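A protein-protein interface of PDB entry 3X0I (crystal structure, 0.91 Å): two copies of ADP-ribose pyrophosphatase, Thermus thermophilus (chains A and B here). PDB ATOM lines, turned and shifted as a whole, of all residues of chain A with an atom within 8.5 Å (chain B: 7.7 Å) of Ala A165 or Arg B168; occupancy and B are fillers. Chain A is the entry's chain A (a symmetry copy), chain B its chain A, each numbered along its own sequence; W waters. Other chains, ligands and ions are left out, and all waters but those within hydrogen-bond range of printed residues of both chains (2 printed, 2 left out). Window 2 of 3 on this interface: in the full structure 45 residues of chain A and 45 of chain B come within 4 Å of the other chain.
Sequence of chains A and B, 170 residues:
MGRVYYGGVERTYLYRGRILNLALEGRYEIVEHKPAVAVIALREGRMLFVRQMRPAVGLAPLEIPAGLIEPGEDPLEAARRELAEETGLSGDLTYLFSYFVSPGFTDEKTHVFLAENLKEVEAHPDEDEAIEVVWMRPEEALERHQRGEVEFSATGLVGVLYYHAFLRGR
O of Val A160 sits at hydrogen-bond distance from ND1 of His A164 (2.8 Å). The backbone carbonyl oxygen (O) of Val B160 is in hydrogen-bond range of a ring nitrogen (ND1) of His B164. NH2 of Arg A168 lies within hydrogen-bond range of O of His A164, 3.2 Å away. The backbone carbonyl oxygen (O) of His B164 is in hydrogen-bond range of the guanidinium group (NH2) of Arg B168, 3.2 Å away.
Leu B161 touches Val A158 (CD1 to O, 3.9 Å). Leu A161 touches Leu B161 (CB to CB, 3.7 Å). Leu A161 touches Ala B165 (O to CB, 3.9 Å). Ala B165 touches His A164. Phe B166 touches His A164 (CZ to CD2, 3.7 Å). Ala A165 touches Leu B161 (CB to O, 3.9 Å). CA of Ala A165 touches CA of Ala B165, at 3.7 Å. Arg B168 touches Ala A165. CE1 of Phe A166 touches CD2 of Leu B161, 3.98 Å away. Arg A168 touches Ala B165.
Of chain B, only Leu B161, His B164, Ala B165 and Arg B168 come within 4 Å of Ala A165. Of chain A, only Ala A165 comes within 4 Å of Arg B168. Printed residues of chain B within 4 Å of Leu A161: Leu B161 (3.7 Å), Ala B165 (3.9 Å) and Phe B166 (3.98 Å). Of the printed residues of chain B, Val A158 touches Leu B161. Of the printed residues of chain B, Arg A168 touches Ala B165. Of the printed residues of chain B, Phe A166 touches Leu B161 (3.98 Å) and His B164 (3.7 Å).
Of the 12 printed residues of chain A, 6 touch a printed residue of chain B. Printed residues of chain A that touch a printed residue of chain B: Val A158, Leu A161, His A164, Ala A165, Phe A166 and Arg A168. Hydrophobic or aromatic side chains of chain A that line the printed part of chain B: Val A158, Leu A161, His A164, Ala A165 and Phe A166. Hydrophobic or aromatic side chains of chain B within 4 Å of the printed part of chain A: Leu B161, His B164, Ala B165 and Phe B166.
Leu A161 touches Ala B165, and with the chains exchanged Ala A165 touches Leu B161. His A164 touches Phe B166, and with the chains exchanged Phe A166 touches His B164. Ala B165 touches its own counterpart, Ala A165. Ala A165 touches Arg B168, and with the chains exchanged Arg A168 touches Ala B165.
Water W2 lies within hydrogen-bond range of the backbone carbonyl oxygen of Ala A165 (3.2 Å) and the guanidinium group of Arg B168 (3.2 Å). Water W1 lies within hydrogen-bond range of O of Ala B165 (3.2 Å) and NH2 of Arg A168 (3.2 Å).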
ATOM      1  N   PHE A  97      -8.639   4.415  18.837  1.00  0.00           N
ATOM      2  CA  PHE A  97      -9.664   3.531  19.410  1.00  0.00           C
ATOM      3  C   PHE A  97      -8.993   2.194  19.710  1.00  0.00           C
ATOM      4  O   PHE A  97      -7.836   1.965  19.335  1.00  0.00           O
ATOM      5  CB  PHE A  97     -10.900   3.356  18.495  1.00  0.00           C
ATOM      6  CG  PHE A  97     -10.587   3.244  17.036  1.00  0.00           C
ATOM      7  CD1 PHE A  97     -11.116   4.186  16.139  1.00  0.00           C
ATOM      8  CD2 PHE A  97      -9.784   2.222  16.500  1.00  0.00           C
ATOM      9  CE1 PHE A  97     -10.838   4.119  14.759  1.00  0.00           C
ATOM     10  CE2 PHE A  97      -9.479   2.172  15.141  1.00  0.00           C
ATOM     11  CZ  PHE A  97      -9.996   3.119  14.256  1.00  0.00           C
ATOM     12  N   VAL A 158      -8.849  -3.022   9.587  1.00  0.00           N
ATOM     13  CA  VAL A 158      -9.184  -1.793  10.312  1.00  0.00           C
ATOM     14  C   VAL A 158      -8.510  -0.610   9.650  1.00  0.00           C
ATOM     15  O   VAL A 158      -9.141   0.450   9.479  1.00  0.00           O
ATOM     16  CB  VAL A 158      -8.826  -1.953  11.801  1.00  0.00           C
ATOM     17  CG1 VAL A 158      -8.740  -0.604  12.495  1.00  0.00           C
ATOM     18  CG2 VAL A 158      -9.815  -2.869  12.481  1.00  0.00           C
ATOM     19  N   GLY A 159      -7.220  -0.732   9.267  1.00  0.00           N
ATOM     20  CA  GLY A 159      -6.576   0.365   8.604  1.00  0.00           C
ATOM     21  C   GLY A 159      -7.286   0.763   7.290  1.00  0.00           C
ATOM     22  O   GLY A 159      -7.518   1.940   7.022  1.00  0.00           O
ATOM     23  N   VAL A 160      -7.597  -0.247   6.475  1.00  0.00           N
ATOM     24  CA  VAL A 160      -8.269   0.024   5.200  1.00  0.00           C
ATOM     25  C   VAL A 160      -9.610   0.700   5.427  1.00  0.00           C
ATOM     26  O   VAL A 160      -9.973   1.673   4.711  1.00  0.00           O
ATOM     27  CB  VAL A 160      -8.418  -1.283   4.411  1.00  0.00           C
ATOM     28  CG1 VAL A 160      -9.382  -1.150   3.252  1.00  0.00           C
ATOM     29  CG2 VAL A 160      -7.042  -1.754   3.888  1.00  0.00           C
ATOM     30  N   LEU A 161     -10.407   0.191   6.361  1.00  0.00           N
ATOM     31  CA  LEU A 161     -11.729   0.772   6.595  1.00  0.00           C
ATOM     32  C   LEU A 161     -11.620   2.183   7.192  1.00  0.00           C
ATOM     33  O   LEU A 161     -12.373   3.074   6.798  1.00  0.00           O
ATOM     34  CB  LEU A 161     -12.573  -0.133   7.468  1.00  0.00           C
ATOM     35  CG  LEU A 161     -12.884  -1.496   6.863  1.00  0.00           C
ATOM     36  CD1 LEU A 161     -13.659  -2.345   7.886  1.00  0.00           C
ATOM     37  CD2 LEU A 161     -13.675  -1.370   5.554  1.00  0.00           C
ATOM     38  N   TYR A 162     -10.696   2.378   8.138  1.00  0.00           N
ATOM     39  CA  TYR A 162     -10.525   3.705   8.691  1.00  0.00           C
ATOM     40  C   TYR A 162     -10.145   4.711   7.603  1.00  0.00           C
ATOM     41  O   TYR A 162     -10.667   5.827   7.586  1.00  0.00           O
ATOM     42  CB  TYR A 162      -9.413   3.644   9.784  1.00  0.00           C
ATOM     43  CG  TYR A 162      -9.233   5.018  10.432  1.00  0.00           C
ATOM     44  CD1 TYR A 162     -10.048   5.415  11.447  1.00  0.00           C
ATOM     45  CD2 TYR A 162      -8.247   5.888   9.950  1.00  0.00           C
ATOM     46  CE1 TYR A 162      -9.941   6.690  12.051  1.00  0.00           C
ATOM     47  CE2 TYR A 162      -8.137   7.136  10.503  1.00  0.00           C
ATOM     48  CZ  TYR A 162      -8.948   7.522  11.531  1.00  0.00           C
ATOM     49  OH  TYR A 162      -8.820   8.803  12.068  1.00  0.00           O
ATOM     50  N   TYR A 163      -9.227   4.327   6.718  1.00  0.00           N
ATOM     51  CA  TYR A 163      -8.892   5.229   5.628  1.00  0.00           C
ATOM     52  C   TYR A 163     -10.114   5.615   4.808  1.00  0.00           C
ATOM     53  O   TYR A 163     -10.332   6.780   4.494  1.00  0.00           O
ATOM     54  CB  TYR A 163      -7.842   4.533   4.708  1.00  0.00           C
ATOM     55  CG  TYR A 163      -7.764   5.198   3.342  1.00  0.00           C
ATOM     56  CD1 TYR A 163      -6.928   6.308   3.132  1.00  0.00           C
ATOM     57  CD2 TYR A 163      -8.466   4.689   2.245  1.00  0.00           C
ATOM     58  CE1 TYR A 163      -6.845   6.903   1.878  1.00  0.00           C
ATOM     59  CE2 TYR A 163      -8.415   5.267   0.997  1.00  0.00           C
ATOM     60  CZ  TYR A 163      -7.590   6.365   0.818  1.00  0.00           C
ATOM     61  OH  TYR A 163      -7.503   6.954  -0.439  1.00  0.00           O
ATOM     62  N   HIS A 164     -10.897   4.607   4.414  1.00  0.00           N
ATOM     63  CA  HIS A 164     -12.040   4.922   3.545  1.00  0.00           C
ATOM     64  C   HIS A 164     -13.066   5.777   4.279  1.00  0.00           C
ATOM     65  O   HIS A 164     -13.709   6.605   3.662  1.00  0.00           O
ATOM     66  CB  HIS A 164     -12.686   3.633   3.014  1.00  0.00           C
ATOM     67  CG  HIS A 164     -11.967   2.956   1.912  1.00  0.00           C
ATOM     68  ND1 HIS A 164     -10.943   2.045   2.099  1.00  0.00           N
ATOM     69  CD2 HIS A 164     -12.152   3.066   0.554  1.00  0.00           C
ATOM     70  CE1 HIS A 164     -10.502   1.634   0.863  1.00  0.00           C
ATOM     71  NE2 HIS A 164     -11.217   2.218  -0.083  1.00  0.00           N
ATOM     72  N   ALA A 165     -13.183   5.596   5.591  1.00  0.00           N
ATOM     73  CA  ALA A 165     -14.135   6.363   6.361  1.00  0.00           C
ATOM     74  C   ALA A 165     -13.675   7.822   6.627  1.00  0.00           C
ATOM     75  O   ALA A 165     -14.531   8.724   6.528  1.00  0.00           O
ATOM     76  CB  ALA A 165     -14.346   5.688   7.735  1.00  0.00           C
ATOM     77  N   PHE A 166     -12.410   8.032   6.899  1.00  0.00           N
ATOM     78  CA  PHE A 166     -11.998   9.286   7.510  1.00  0.00           C
ATOM     79  C   PHE A 166     -10.817   9.976   6.815  1.00  0.00           C
ATOM     80  O   PHE A 166     -10.559  11.133   7.155  1.00  0.00           O
ATOM     81  CB  PHE A 166     -11.639   9.089   8.979  1.00  0.00           C
ATOM     82  CG  PHE A 166     -12.803   8.600   9.795  1.00  0.00           C
ATOM     83  CD1 PHE A 166     -12.787   7.394  10.399  1.00  0.00           C
ATOM     84  CD2 PHE A 166     -13.962   9.373   9.896  1.00  0.00           C
ATOM     85  CE1 PHE A 166     -13.878   6.935  11.144  1.00  0.00           C
ATOM     86  CE2 PHE A 166     -15.020   8.933  10.683  1.00  0.00           C
ATOM     87  CZ  PHE A 166     -15.013   7.689  11.305  1.00  0.00           C
ATOM     88  N   LEU A 167     -10.095   9.323   5.911  1.00  0.00           N
ATOM     89  CA  LEU A 167      -8.844   9.909   5.405  1.00  0.00           C
ATOM     90  C   LEU A 167      -8.859  10.242   3.920  1.00  0.00           C
ATOM     91  O   LEU A 167      -7.819  10.589   3.380  1.00  0.00           O
ATOM     92  CB  LEU A 167      -7.660   8.959   5.713  1.00  0.00           C
ATOM     93  CG  LEU A 167      -7.358   8.637   7.150  1.00  0.00           C
ATOM     94  CD1 LEU A 167      -6.163   7.701   7.291  1.00  0.00           C
ATOM     95  CD2 LEU A 167      -7.088   9.875   7.960  1.00  0.00           C
ATOM     96  N   ARG A 168      -9.984  10.151   3.296  1.00  0.00           N
ATOM     97  CA  ARG A 168     -10.018  10.563   1.873  1.00  0.00           C
ATOM     98  C   ARG A 168     -10.201  12.087   1.708  1.00  0.00           C
ATOM     99  O   ARG A 168      -9.701  12.451   0.616  1.00  0.00           O
ATOM    100  CB  ARG A 168     -11.120   9.680   1.184  1.00  0.00           C
ATOM    101  CG  ARG A 168     -10.652   8.196   1.194  1.00  0.00           C
ATOM    102  CD  ARG A 168     -11.387   7.388   0.178  1.00  0.00           C
ATOM    103  NE  ARG A 168     -12.757   7.137   0.684  1.00  0.00           N
ATOM    104  CZ  ARG A 168     -13.770   6.470   0.107  1.00  0.00           C
ATOM    105  NH1 ARG A 168     -13.544   6.039  -1.133  1.00  0.00           N
ATOM    106  NH2 ARG A 168     -14.885   6.326   0.747  1.00  0.00           N
ATOM    107  N   LEU B  42     -27.847  -2.417   9.067  1.00  0.00           N
ATOM    108  CA  LEU B  42     -28.235  -1.039   9.327  1.00  0.00           C
ATOM    109  C   LEU B  42     -29.757  -1.027   9.117  1.00  0.00           C
ATOM    110  O   LEU B  42     -30.215  -1.491   8.076  1.00  0.00           O
ATOM    111  CB  LEU B  42     -27.481  -0.078   8.406  1.00  0.00           C
ATOM    112  CG  LEU B  42     -27.452   1.399   8.811  1.00  0.00           C
ATOM    113  CD1 LEU B  42     -26.503   1.581   9.988  1.00  0.00           C
ATOM    114  CD2 LEU B  42     -27.042   2.287   7.643  1.00  0.00           C
ATOM    115  N   PRO B 138     -24.205   4.162  14.530  1.00  0.00           N
ATOM    116  CA  PRO B 138     -22.773   3.974  14.662  1.00  0.00           C
ATOM    117  C   PRO B 138     -22.022   5.186  15.159  1.00  0.00           C
ATOM    118  O   PRO B 138     -20.968   5.049  15.794  1.00  0.00           O
ATOM    119  CB  PRO B 138     -22.310   3.590  13.220  1.00  0.00           C
ATOM    120  CG  PRO B 138     -23.536   2.984  12.636  1.00  0.00           C
ATOM    121  CD  PRO B 138     -24.720   3.765  13.237  1.00  0.00           C
ATOM    122  N   GLU B 139     -22.545   6.377  14.839  1.00  0.00           N
ATOM    123  CA  GLU B 139     -21.860   7.598  15.305  1.00  0.00           C
ATOM    124  C   GLU B 139     -21.903   7.634  16.817  1.00  0.00           C
ATOM    125  O   GLU B 139     -20.971   8.100  17.452  1.00  0.00           O
ATOM    126  CB  GLU B 139     -22.651   8.800  14.737  1.00  0.00           C
ATOM    127  CG  GLU B 139     -22.588   8.941  13.221  1.00  0.00           C
ATOM    128  CD  GLU B 139     -23.669   8.200  12.437  1.00  0.00           C
ATOM    129  OE1 GLU B 139     -24.344   7.323  12.983  1.00  0.00           O
ATOM    130  OE2 GLU B 139     -23.799   8.541  11.253  1.00  0.00           O
ATOM    131  N   VAL B 160     -18.659  -0.504  12.651  1.00  0.00           N
ATOM    132  CA  VAL B 160     -18.693   0.960  12.732  1.00  0.00           C
ATOM    133  C   VAL B 160     -17.882   1.584  11.609  1.00  0.00           C
ATOM    134  O   VAL B 160     -18.321   2.579  10.970  1.00  0.00           O
ATOM    135  CB  VAL B 160     -18.195   1.410  14.111  1.00  0.00           C
ATOM    136  CG1 VAL B 160     -17.888   2.891  14.158  1.00  0.00           C
ATOM    137  CG2 VAL B 160     -19.236   1.060  15.198  1.00  0.00           C
ATOM    138  N   LEU B 161     -16.674   1.084  11.369  1.00  0.00           N
ATOM    139  CA  LEU B 161     -15.829   1.673  10.331  1.00  0.00           C
ATOM    140  C   LEU B 161     -16.413   1.427   8.932  1.00  0.00           C
ATOM    141  O   LEU B 161     -16.390   2.327   8.092  1.00  0.00           O
ATOM    142  CB  LEU B 161     -14.407   1.161  10.434  1.00  0.00           C
ATOM    143  CG  LEU B 161     -13.689   1.524  11.727  1.00  0.00           C
ATOM    144  CD1 LEU B 161     -12.298   0.864  11.742  1.00  0.00           C
ATOM    145  CD2 LEU B 161     -13.569   3.044  11.903  1.00  0.00           C
ATOM    146  N   TYR B 162     -16.923   0.216   8.685  1.00  0.00           N
ATOM    147  CA  TYR B 162     -17.529  -0.042   7.396  1.00  0.00           C
ATOM    148  C   TYR B 162     -18.705   0.904   7.141  1.00  0.00           C
ATOM    149  O   TYR B 162     -18.849   1.422   6.032  1.00  0.00           O
ATOM    150  CB  TYR B 162     -18.011  -1.526   7.366  1.00  0.00           C
ATOM    151  CG  TYR B 162     -18.617  -1.858   6.001  1.00  0.00           C
ATOM    152  CD1 TYR B 162     -17.816  -2.217   4.961  1.00  0.00           C
ATOM    153  CD2 TYR B 162     -20.000  -1.752   5.811  1.00  0.00           C
ATOM    154  CE1 TYR B 162     -18.329  -2.497   3.671  1.00  0.00           C
ATOM    155  CE2 TYR B 162     -20.519  -1.996   4.568  1.00  0.00           C
ATOM    156  CZ  TYR B 162     -19.713  -2.372   3.532  1.00  0.00           C
ATOM    157  OH  TYR B 162     -20.268  -2.605   2.274  1.00  0.00           O
ATOM    158  N   TYR B 163     -19.548   1.106   8.150  1.00  0.00           N
ATOM    159  CA  TYR B 163     -20.637   2.053   7.968  1.00  0.00           C
ATOM    160  C   TYR B 163     -20.135   3.433   7.572  1.00  0.00           C
ATOM    161  O   TYR B 163     -20.647   4.060   6.652  1.00  0.00           O
ATOM    162  CB  TYR B 163     -21.443   2.150   9.300  1.00  0.00           C
ATOM    163  CG  TYR B 163     -22.303   3.404   9.345  1.00  0.00           C
ATOM    164  CD1 TYR B 163     -23.594   3.409   8.788  1.00  0.00           C
ATOM    165  CD2 TYR B 163     -21.865   4.562   9.995  1.00  0.00           C
ATOM    166  CE1 TYR B 163     -24.385   4.551   8.846  1.00  0.00           C
ATOM    167  CE2 TYR B 163     -22.620   5.711  10.053  1.00  0.00           C
ATOM    168  CZ  TYR B 163     -23.886   5.692   9.490  1.00  0.00           C
ATOM    169  OH  TYR B 163     -24.678   6.833   9.555  1.00  0.00           O
ATOM    170  N   HIS B 164     -19.145   3.932   8.317  1.00  0.00           N
ATOM    171  CA  HIS B 164     -18.687   5.298   8.027  1.00  0.00           C
ATOM    172  C   HIS B 164     -18.043   5.380   6.649  1.00  0.00           C
ATOM    173  O   HIS B 164     -18.153   6.399   5.994  1.00  0.00           O
ATOM    174  CB  HIS B 164     -17.713   5.783   9.113  1.00  0.00           C
ATOM    175  CG  HIS B 164     -18.327   6.202  10.393  1.00  0.00           C
ATOM    176  ND1 HIS B 164     -18.627   5.336  11.429  1.00  0.00           N
ATOM    177  CD2 HIS B 164     -18.698   7.458  10.810  1.00  0.00           C
ATOM    178  CE1 HIS B 164     -19.197   6.064  12.446  1.00  0.00           C
ATOM    179  NE2 HIS B 164     -19.241   7.342  12.111  1.00  0.00           N
ATOM    180  N   ALA B 165     -17.410   4.297   6.208  1.00  0.00           N
ATOM    181  CA  ALA B 165     -16.769   4.292   4.913  1.00  0.00           C
ATOM    182  C   ALA B 165     -17.770   4.161   3.733  1.00  0.00           C
ATOM    183  O   ALA B 165     -17.570   4.866   2.725  1.00  0.00           O
ATOM    184  CB  ALA B 165     -15.795   3.095   4.827  1.00  0.00           C
ATOM    185  N   PHE B 166     -18.791   3.350   3.875  1.00  0.00           N
ATOM    186  CA  PHE B 166     -19.533   2.907   2.704  1.00  0.00           C
ATOM    187  C   PHE B 166     -21.056   3.055   2.823  1.00  0.00           C
ATOM    188  O   PHE B 166     -21.720   2.895   1.796  1.00  0.00           O
ATOM    189  CB  PHE B 166     -19.219   1.453   2.373  1.00  0.00           C
ATOM    190  CG  PHE B 166     -17.768   1.238   2.042  1.00  0.00           C
ATOM    191  CD1 PHE B 166     -16.975   0.459   2.804  1.00  0.00           C
ATOM    192  CD2 PHE B 166     -17.193   1.899   0.952  1.00  0.00           C
ATOM    193  CE1 PHE B 166     -15.622   0.275   2.501  1.00  0.00           C
ATOM    194  CE2 PHE B 166     -15.862   1.667   0.628  1.00  0.00           C
ATOM    195  CZ  PHE B 166     -15.036   0.870   1.412  1.00  0.00           C
ATOM    196  N   LEU B 167     -21.616   3.312   4.000  1.00  0.00           N
ATOM    197  CA  LEU B 167     -23.078   3.243   4.149  1.00  0.00           C
ATOM    198  C   LEU B 167     -23.740   4.571   4.492  1.00  0.00           C
ATOM    199  O   LEU B 167     -24.926   4.584   4.784  1.00  0.00           O
ATOM    200  CB  LEU B 167     -23.445   2.187   5.222  1.00  0.00           C
ATOM    201  CG  LEU B 167     -23.034   0.761   4.990  1.00  0.00           C
ATOM    202  CD1 LEU B 167     -23.473  -0.158   6.125  1.00  0.00           C
ATOM    203  CD2 LEU B 167     -23.587   0.217   3.700  1.00  0.00           C
ATOM    204  N   ARG B 168     -23.011   5.633   4.446  1.00  0.00           N
ATOM    205  CA  ARG B 168     -23.676   6.936   4.690  1.00  0.00           C
ATOM    206  C   ARG B 168     -24.343   7.499   3.417  1.00  0.00           C
ATOM    207  O   ARG B 168     -25.297   8.248   3.744  1.00  0.00           O
ATOM    208  CB  ARG B 168     -22.593   7.868   5.345  1.00  0.00           C
ATOM    209  CG  ARG B 168     -22.226   7.301   6.746  1.00  0.00           C
ATOM    210  CD  ARG B 168     -21.585   8.342   7.603  1.00  0.00           C
ATOM    211  NE  ARG B 168     -20.196   8.543   7.130  1.00  0.00           N
ATOM    212  CZ  ARG B 168     -19.253   9.384   7.587  1.00  0.00           C
ATOM    213  NH1 ARG B 168     -19.644  10.218   8.550  1.00  0.00           N
ATOM    214  NH2 ARG B 168     -18.073   9.370   7.057  1.00  0.00           N
HETATM  215  O   HOH W   1     -17.721   5.337  -0.404  1.00  0.00           O
HETATM  216  O   HOH W   2     -15.714  11.528   7.402  1.00  0.00           O
